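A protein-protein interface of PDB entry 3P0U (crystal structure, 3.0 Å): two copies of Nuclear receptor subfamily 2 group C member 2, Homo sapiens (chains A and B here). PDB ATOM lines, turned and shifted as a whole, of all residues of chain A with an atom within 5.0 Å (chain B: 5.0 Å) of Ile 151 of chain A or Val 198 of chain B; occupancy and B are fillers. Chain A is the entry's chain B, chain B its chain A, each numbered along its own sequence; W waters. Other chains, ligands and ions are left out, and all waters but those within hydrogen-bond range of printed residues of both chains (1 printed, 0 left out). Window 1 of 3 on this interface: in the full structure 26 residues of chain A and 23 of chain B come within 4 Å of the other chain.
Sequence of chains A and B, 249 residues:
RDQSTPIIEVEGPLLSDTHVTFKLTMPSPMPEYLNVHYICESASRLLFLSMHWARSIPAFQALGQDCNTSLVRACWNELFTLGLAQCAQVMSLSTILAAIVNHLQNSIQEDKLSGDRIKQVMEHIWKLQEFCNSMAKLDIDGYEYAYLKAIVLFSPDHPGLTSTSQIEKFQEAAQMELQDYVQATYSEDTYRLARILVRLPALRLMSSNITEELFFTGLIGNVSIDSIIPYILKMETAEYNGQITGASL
Water W1 lies within hydrogen-bond range of OD1 of Asp 157 of chain A, O of Val 198 of chain B and OG of Ser 155 of chain A.
Of the 15 printed residues of chain A, 5 touch a printed residue of chain B. Printed residues of chain A that touch a printed residue of chain B: Ile 151, Asp 157, Gln 171, Gln 175 and Leu 197. Hydrophobic or aromatic side chains of chain B within 4 Å of the printed part of chain A: Ala 194, Leu 197 and Val 198. Among the printed residues, 7 pairs touch across the chains. Among the printed residues, Asp or Glu carboxylates within 4 Å of a Lys or Arg side-chain nitrogen of the other chain: Asp 157 of chain A with Arg 199 of chain B.
NH2 of Arg 199 of chain B is in salt-bridge range of OD2 of Asp 157 of chain A (2.8 Å).
CG2 of Ile 151 of chain A touches CG1 of Val 198 of chain B, at 3.4 Å. Gln 171 of chain A touches Val 198 of chain B. Gln 175 of chain A touches Arg 195 of chain B. Val 198 of chain B touches Gln 175 of chain A. Ala 194 of chain B touches Leu 197 of chain A. CD1 of Leu 197 of chain B touches CD1 of Leu 197 of chain A, 3.96 Å away.
The side-chain hydroxyl (OG) of Ser 155 of chain A is in hydrogen-bond range of the side-chain carboxylate (OD1) of Asp 157 of chain A, at 3.3 Å. O of Ile 151 of chain A lies close to OE1 of Gln 171 of chain A.
Leu 197 of chain B touches its own counterpart, Leu 197 of chain A. Of the 7 pairs that touch across the chains among the printed residues, 1 has its exchanged pair printed and touching as well.
Tyr 147 of chain A touches none of the printed residues of chain B. Ile 151 of chain A touches just one residue of chain B: Val 198 (3.4 Å). Of the printed residues of chain B, Gln 171 of chain A touches Val 198. Printed residues of chain B within 4 Å of Gln 175 of chain A: Arg 195 (3.2 Å) and Val 198 (3.6 Å). Of the printed residues of chain B, Leu 197 of chain A touches Ala 194 (3.5 Å) and Leu 197 (3.96 Å). Of the printed residues of chain A, Arg 195 of chain B touches Gln 175 (3.2 Å). Val 198 of chain B touches just these residues of chain A: Ile 151 (3.4 Å), Gln 171 (3.2 Å) and Gln 175 (3.6 Å). Of the printed residues of chain A, Arg 199 of chain B touches Asp 157.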
ATOM      1  N   TYR A 147     -18.365  -5.192  -0.457  1.00  0.00           N
ATOM      2  CA  TYR A 147     -19.687  -4.635  -0.585  1.00  0.00           C
ATOM      3  C   TYR A 147     -20.735  -5.535   0.073  1.00  0.00           C
ATOM      4  O   TYR A 147     -21.675  -5.043   0.700  1.00  0.00           O
ATOM      5  CB  TYR A 147     -20.031  -4.347  -2.050  1.00  0.00           C
ATOM      6  CG  TYR A 147     -19.485  -3.043  -2.567  1.00  0.00           C
ATOM      7  CD1 TYR A 147     -19.522  -1.888  -1.789  1.00  0.00           C
ATOM      8  CD2 TYR A 147     -18.944  -2.957  -3.838  1.00  0.00           C
ATOM      9  CE1 TYR A 147     -19.016  -0.681  -2.245  1.00  0.00           C
ATOM     10  CE2 TYR A 147     -18.436  -1.744  -4.325  1.00  0.00           C
ATOM     11  CZ  TYR A 147     -18.482  -0.601  -3.515  1.00  0.00           C
ATOM     12  OH  TYR A 147     -18.015   0.627  -3.955  1.00  0.00           O
ATOM     13  N   LEU A 148     -20.577  -6.843  -0.047  1.00  0.00           N
ATOM     14  CA  LEU A 148     -21.442  -7.739   0.687  1.00  0.00           C
ATOM     15  C   LEU A 148     -21.216  -7.574   2.195  1.00  0.00           C
ATOM     16  O   LEU A 148     -22.107  -7.831   2.987  1.00  0.00           O
ATOM     17  CB  LEU A 148     -21.208  -9.185   0.277  1.00  0.00           C
ATOM     18  CG  LEU A 148     -21.643  -9.591  -1.126  1.00  0.00           C
ATOM     19  CD1 LEU A 148     -20.999 -10.901  -1.472  1.00  0.00           C
ATOM     20  CD2 LEU A 148     -23.165  -9.717  -1.233  1.00  0.00           C
ATOM     21  N   LYS A 149     -20.032  -7.154   2.608  1.00  0.00           N
ATOM     22  CA  LYS A 149     -19.782  -6.980   4.017  1.00  0.00           C
ATOM     23  C   LYS A 149     -20.482  -5.722   4.476  1.00  0.00           C
ATOM     24  O   LYS A 149     -20.762  -5.542   5.655  1.00  0.00           O
ATOM     25  CB  LYS A 149     -18.292  -6.880   4.306  1.00  0.00           C
ATOM     26  CG  LYS A 149     -17.485  -8.158   4.081  1.00  0.00           C
ATOM     27  CD  LYS A 149     -16.141  -8.025   4.800  1.00  0.00           C
ATOM     28  CE  LYS A 149     -15.274  -9.285   4.825  1.00  0.00           C
ATOM     29  NZ  LYS A 149     -14.762  -9.644   3.510  1.00  0.00           N
ATOM     30  N   ALA A 150     -20.746  -4.829   3.539  1.00  0.00           N
ATOM     31  CA  ALA A 150     -21.458  -3.596   3.868  1.00  0.00           C
ATOM     32  C   ALA A 150     -22.922  -3.926   4.064  1.00  0.00           C
ATOM     33  O   ALA A 150     -23.545  -3.468   5.024  1.00  0.00           O
ATOM     34  CB  ALA A 150     -21.292  -2.559   2.769  1.00  0.00           C
ATOM     35  N   ILE A 151     -23.469  -4.725   3.162  1.00  0.00           N
ATOM     36  CA  ILE A 151     -24.882  -5.103   3.273  1.00  0.00           C
ATOM     37  C   ILE A 151     -25.127  -5.783   4.648  1.00  0.00           C
ATOM     38  O   ILE A 151     -26.176  -5.612   5.301  1.00  0.00           O
ATOM     39  CB  ILE A 151     -25.342  -6.076   2.126  1.00  0.00           C
ATOM     40  CG1 ILE A 151     -24.873  -5.590   0.720  1.00  0.00           C
ATOM     41  CG2 ILE A 151     -26.857  -6.326   2.205  1.00  0.00           C
ATOM     42  CD1 ILE A 151     -25.147  -4.137   0.394  1.00  0.00           C
ATOM     43  N   VAL A 152     -24.115  -6.528   5.069  1.00  0.00           N
ATOM     44  CA  VAL A 152     -24.149  -7.251   6.294  1.00  0.00           C
ATOM     45  C   VAL A 152     -24.000  -6.262   7.445  1.00  0.00           C
ATOM     46  O   VAL A 152     -24.796  -6.238   8.390  1.00  0.00           O
ATOM     47  CB  VAL A 152     -23.006  -8.318   6.276  1.00  0.00           C
ATOM     48  CG1 VAL A 152     -22.787  -8.951   7.634  1.00  0.00           C
ATOM     49  CG2 VAL A 152     -23.319  -9.407   5.293  1.00  0.00           C
ATOM     50  N   LEU A 153     -22.981  -5.432   7.350  1.00  0.00           N
ATOM     51  CA  LEU A 153     -22.649  -4.506   8.441  1.00  0.00           C
ATOM     52  C   LEU A 153     -23.824  -3.612   8.784  1.00  0.00           C
ATOM     53  O   LEU A 153     -24.271  -3.570   9.937  1.00  0.00           O
ATOM     54  CB  LEU A 153     -21.422  -3.625   8.076  1.00  0.00           C
ATOM     55  CG  LEU A 153     -20.716  -2.853   9.200  1.00  0.00           C
ATOM     56  CD1 LEU A 153     -20.341  -3.767  10.320  1.00  0.00           C
ATOM     57  CD2 LEU A 153     -19.462  -2.201   8.674  1.00  0.00           C
ATOM     58  N   PHE A 154     -24.328  -2.937   7.750  1.00  0.00           N
ATOM     59  CA  PHE A 154     -25.429  -1.983   7.879  1.00  0.00           C
ATOM     60  C   PHE A 154     -26.819  -2.677   7.790  1.00  0.00           C
ATOM     61  O   PHE A 154     -27.620  -2.354   6.923  1.00  0.00           O
ATOM     62  CB  PHE A 154     -25.273  -0.858   6.836  1.00  0.00           C
ATOM     63  CG  PHE A 154     -23.903  -0.194   6.861  1.00  0.00           C
ATOM     64  CD1 PHE A 154     -23.495   0.581   7.955  1.00  0.00           C
ATOM     65  CD2 PHE A 154     -23.007  -0.370   5.809  1.00  0.00           C
ATOM     66  CE1 PHE A 154     -22.235   1.167   7.999  1.00  0.00           C
ATOM     67  CE2 PHE A 154     -21.737   0.194   5.862  1.00  0.00           C
ATOM     68  CZ  PHE A 154     -21.355   0.976   6.959  1.00  0.00           C
ATOM     69  N   SER A 155     -27.108  -3.615   8.697  1.00  0.00           N
ATOM     70  CA  SER A 155     -28.382  -4.308   8.659  1.00  0.00           C
ATOM     71  C   SER A 155     -29.300  -3.626   9.645  1.00  0.00           C
ATOM     72  O   SER A 155     -28.914  -3.396  10.778  1.00  0.00           O
ATOM     73  CB  SER A 155     -28.221  -5.784   8.989  1.00  0.00           C
ATOM     74  OG  SER A 155     -29.384  -6.514   8.632  1.00  0.00           O
ATOM     75  N   ASP A 157     -31.961  -4.833  10.630  1.00  0.00           N
ATOM     76  CA  ASP A 157     -32.672  -5.930  11.254  1.00  0.00           C
ATOM     77  C   ASP A 157     -32.354  -6.042  12.733  1.00  0.00           C
ATOM     78  O   ASP A 157     -33.226  -6.381  13.547  1.00  0.00           O
ATOM     79  CB  ASP A 157     -32.296  -7.217  10.510  1.00  0.00           C
ATOM     80  CG  ASP A 157     -32.693  -7.179   9.019  1.00  0.00           C
ATOM     81  OD1 ASP A 157     -32.275  -8.069   8.228  1.00  0.00           O
ATOM     82  OD2 ASP A 157     -33.452  -6.256   8.638  1.00  0.00           O
ATOM     83  N   GLN A 171     -26.886   0.965   3.768  1.00  0.00           N
ATOM     84  CA  GLN A 171     -27.096  -0.362   3.239  1.00  0.00           C
ATOM     85  C   GLN A 171     -27.722  -0.269   1.908  1.00  0.00           C
ATOM     86  O   GLN A 171     -27.397  -1.077   1.024  1.00  0.00           O
ATOM     87  CB  GLN A 171     -27.966  -1.233   4.123  1.00  0.00           C
ATOM     88  CG  GLN A 171     -27.626  -2.727   3.955  1.00  0.00           C
ATOM     89  CD  GLN A 171     -28.784  -3.639   4.206  1.00  0.00           C
ATOM     90  OE1 GLN A 171     -28.593  -4.851   4.386  1.00  0.00           O
ATOM     91  NE2 GLN A 171     -29.996  -3.086   4.214  1.00  0.00           N
ATOM     92  N   ALA A 174     -24.806   0.731  -0.611  1.00  0.00           N
ATOM     93  CA  ALA A 174     -24.027  -0.457  -0.928  1.00  0.00           C
ATOM     94  C   ALA A 174     -24.796  -1.402  -1.827  1.00  0.00           C
ATOM     95  O   ALA A 174     -24.241  -2.128  -2.636  1.00  0.00           O
ATOM     96  CB  ALA A 174     -23.654  -1.168   0.356  1.00  0.00           C
ATOM     97  N   GLN A 175     -26.096  -1.414  -1.683  1.00  0.00           N
ATOM     98  CA  GLN A 175     -26.878  -2.255  -2.533  1.00  0.00           C
ATOM     99  C   GLN A 175     -26.750  -1.844  -3.977  1.00  0.00           C
ATOM    100  O   GLN A 175     -26.562  -2.679  -4.849  1.00  0.00           O
ATOM    101  CB  GLN A 175     -28.333  -2.194  -2.107  1.00  0.00           C
ATOM    102  CG  GLN A 175     -28.779  -3.372  -1.316  1.00  0.00           C
ATOM    103  CD  GLN A 175     -30.120  -3.117  -0.717  1.00  0.00           C
ATOM    104  OE1 GLN A 175     -31.102  -2.865  -1.428  1.00  0.00           O
ATOM    105  NE2 GLN A 175     -30.182  -3.158   0.619  1.00  0.00           N
ATOM    106  N   LEU A 178     -22.942  -2.131  -5.451  1.00  0.00           N
ATOM    107  CA  LEU A 178     -22.684  -3.561  -5.739  1.00  0.00           C
ATOM    108  C   LEU A 178     -23.335  -3.964  -7.053  1.00  0.00           C
ATOM    109  O   LEU A 178     -22.786  -4.740  -7.819  1.00  0.00           O
ATOM    110  CB  LEU A 178     -23.191  -4.484  -4.605  1.00  0.00           C
ATOM    111  CG  LEU A 178     -23.356  -5.980  -4.994  1.00  0.00           C
ATOM    112  CD1 LEU A 178     -22.036  -6.655  -5.240  1.00  0.00           C
ATOM    113  CD2 LEU A 178     -24.110  -6.804  -4.010  1.00  0.00           C
ATOM    114  N   LEU A 197     -26.505 -12.343  -3.879  1.00  0.00           N
ATOM    115  CA  LEU A 197     -27.372 -11.870  -2.795  1.00  0.00           C
ATOM    116  C   LEU A 197     -28.084 -12.979  -2.060  1.00  0.00           C
ATOM    117  O   LEU A 197     -28.172 -12.915  -0.860  1.00  0.00           O
ATOM    118  CB  LEU A 197     -28.430 -10.910  -3.334  1.00  0.00           C
ATOM    119  CG  LEU A 197     -27.904  -9.535  -3.751  1.00  0.00           C
ATOM    120  CD1 LEU A 197     -29.063  -8.597  -4.152  1.00  0.00           C
ATOM    121  CD2 LEU A 197     -27.048  -8.933  -2.606  1.00  0.00           C
ATOM    122  N   ALA B 194     -32.847  -6.300  -5.933  1.00  0.00           N
ATOM    123  CA  ALA B 194     -31.825  -6.452  -4.927  1.00  0.00           C
ATOM    124  C   ALA B 194     -32.360  -6.009  -3.596  1.00  0.00           C
ATOM    125  O   ALA B 194     -32.063  -6.626  -2.577  1.00  0.00           O
ATOM    126  CB  ALA B 194     -30.589  -5.642  -5.271  1.00  0.00           C
ATOM    127  N   ARG B 195     -33.138  -4.936  -3.591  1.00  0.00           N
ATOM    128  CA  ARG B 195     -33.742  -4.434  -2.334  1.00  0.00           C
ATOM    129  C   ARG B 195     -34.656  -5.505  -1.673  1.00  0.00           C
ATOM    130  O   ARG B 195     -34.756  -5.624  -0.437  1.00  0.00           O
ATOM    131  CB  ARG B 195     -34.547  -3.145  -2.595  1.00  0.00           C
ATOM    132  CG  ARG B 195     -34.133  -1.974  -1.724  1.00  0.00           C
ATOM    133  CD  ARG B 195     -35.266  -0.996  -1.623  1.00  0.00           C
ATOM    134  NE  ARG B 195     -35.797  -0.625  -2.945  1.00  0.00           N
ATOM    135  CZ  ARG B 195     -35.392   0.414  -3.685  1.00  0.00           C
ATOM    136  NH1 ARG B 195     -34.420   1.238  -3.272  1.00  0.00           N
ATOM    137  NH2 ARG B 195     -35.976   0.635  -4.859  1.00  0.00           N
ATOM    138  N   ILE B 196     -35.311  -6.282  -2.528  1.00  0.00           N
ATOM    139  CA  ILE B 196     -36.154  -7.351  -2.090  1.00  0.00           C
ATOM    140  C   ILE B 196     -35.333  -8.543  -1.584  1.00  0.00           C
ATOM    141  O   ILE B 196     -35.631  -9.127  -0.535  1.00  0.00           O
ATOM    142  CB  ILE B 196     -37.066  -7.760  -3.230  1.00  0.00           C
ATOM    143  CG1 ILE B 196     -38.196  -6.750  -3.360  1.00  0.00           C
ATOM    144  CG2 ILE B 196     -37.682  -9.095  -2.988  1.00  0.00           C
ATOM    145  CD1 ILE B 196     -39.312  -7.243  -4.288  1.00  0.00           C
ATOM    146  N   LEU B 197     -34.300  -8.922  -2.314  1.00  0.00           N
ATOM    147  CA  LEU B 197     -33.498 -10.048  -1.884  1.00  0.00           C
ATOM    148  C   LEU B 197     -32.769  -9.787  -0.537  1.00  0.00           C
ATOM    149  O   LEU B 197     -32.476 -10.743   0.242  1.00  0.00           O
ATOM    150  CB  LEU B 197     -32.479 -10.377  -2.951  1.00  0.00           C
ATOM    151  CG  LEU B 197     -33.062 -10.789  -4.284  1.00  0.00           C
ATOM    152  CD1 LEU B 197     -31.951 -11.089  -5.219  1.00  0.00           C
ATOM    153  CD2 LEU B 197     -33.924 -11.987  -4.142  1.00  0.00           C
ATOM    154  N   VAL B 198     -32.466  -8.515  -0.257  1.00  0.00           N
ATOM    155  CA  VAL B 198     -31.776  -8.158   0.994  1.00  0.00           C
ATOM    156  C   VAL B 198     -32.754  -8.184   2.175  1.00  0.00           C
ATOM    157  O   VAL B 198     -32.384  -7.936   3.318  1.00  0.00           O
ATOM    158  CB  VAL B 198     -31.034  -6.785   0.887  1.00  0.00           C
ATOM    159  CG1 VAL B 198     -30.287  -6.418   2.174  1.00  0.00           C
ATOM    160  CG2 VAL B 198     -30.076  -6.856  -0.249  1.00  0.00           C
ATOM    161  N   ARG B 199     -33.993  -8.519   1.915  1.00  0.00           N
ATOM    162  CA  ARG B 199     -34.920  -8.708   3.006  1.00  0.00           C
ATOM    163  C   ARG B 199     -34.880 -10.137   3.554  1.00  0.00           C
ATOM    164  O   ARG B 199     -35.174 -10.364   4.725  1.00  0.00           O
ATOM    165  CB  ARG B 199     -36.338  -8.390   2.523  1.00  0.00           C
ATOM    166  CG  ARG B 199     -36.546  -6.927   2.196  1.00  0.00           C
ATOM    167  CD  ARG B 199     -36.861  -6.200   3.447  1.00  0.00           C
ATOM    168  NE  ARG B 199     -35.643  -5.939   4.168  1.00  0.00           N
ATOM    169  CZ  ARG B 199     -35.495  -6.096   5.469  1.00  0.00           C
ATOM    170  NH1 ARG B 199     -36.489  -6.541   6.210  1.00  0.00           N
ATOM    171  NH2 ARG B 199     -34.330  -5.810   6.032  1.00  0.00           N
ATOM    172  N   LEU B 200     -34.548 -11.097   2.695  1.00  0.00           N
ATOM    173  CA  LEU B 200     -34.576 -12.508   3.090  1.00  0.00           C
ATOM    174  C   LEU B 200     -33.717 -12.834   4.333  1.00  0.00           C
ATOM    175  O   LEU B 200     -34.085 -13.683   5.141  1.00  0.00           O
ATOM    176  CB  LEU B 200     -34.172 -13.417   1.921  1.00  0.00           C
ATOM    177  CG  LEU B 200     -35.118 -13.461   0.711  1.00  0.00           C
ATOM    178  CD1 LEU B 200     -34.469 -14.207  -0.425  1.00  0.00           C
ATOM    179  CD2 LEU B 200     -36.521 -14.078   1.053  1.00  0.00           C
ATOM    180  N   PRO B 201     -32.587 -12.147   4.504  1.00  0.00           N
ATOM    181  CA  PRO B 201     -31.768 -12.472   5.644  1.00  0.00           C
ATOM    182  C   PRO B 201     -32.512 -12.259   6.915  1.00  0.00           C
ATOM    183  O   PRO B 201     -32.269 -12.960   7.867  1.00  0.00           O
ATOM    184  CB  PRO B 201     -30.579 -11.518   5.492  1.00  0.00           C
ATOM    185  CG  PRO B 201     -30.393 -11.488   3.998  1.00  0.00           C
ATOM    186  CD  PRO B 201     -31.850 -11.294   3.563  1.00  0.00           C
HETATM  187  O   HOH W   1     -30.726  -7.915   5.862  1.00  0.00           O
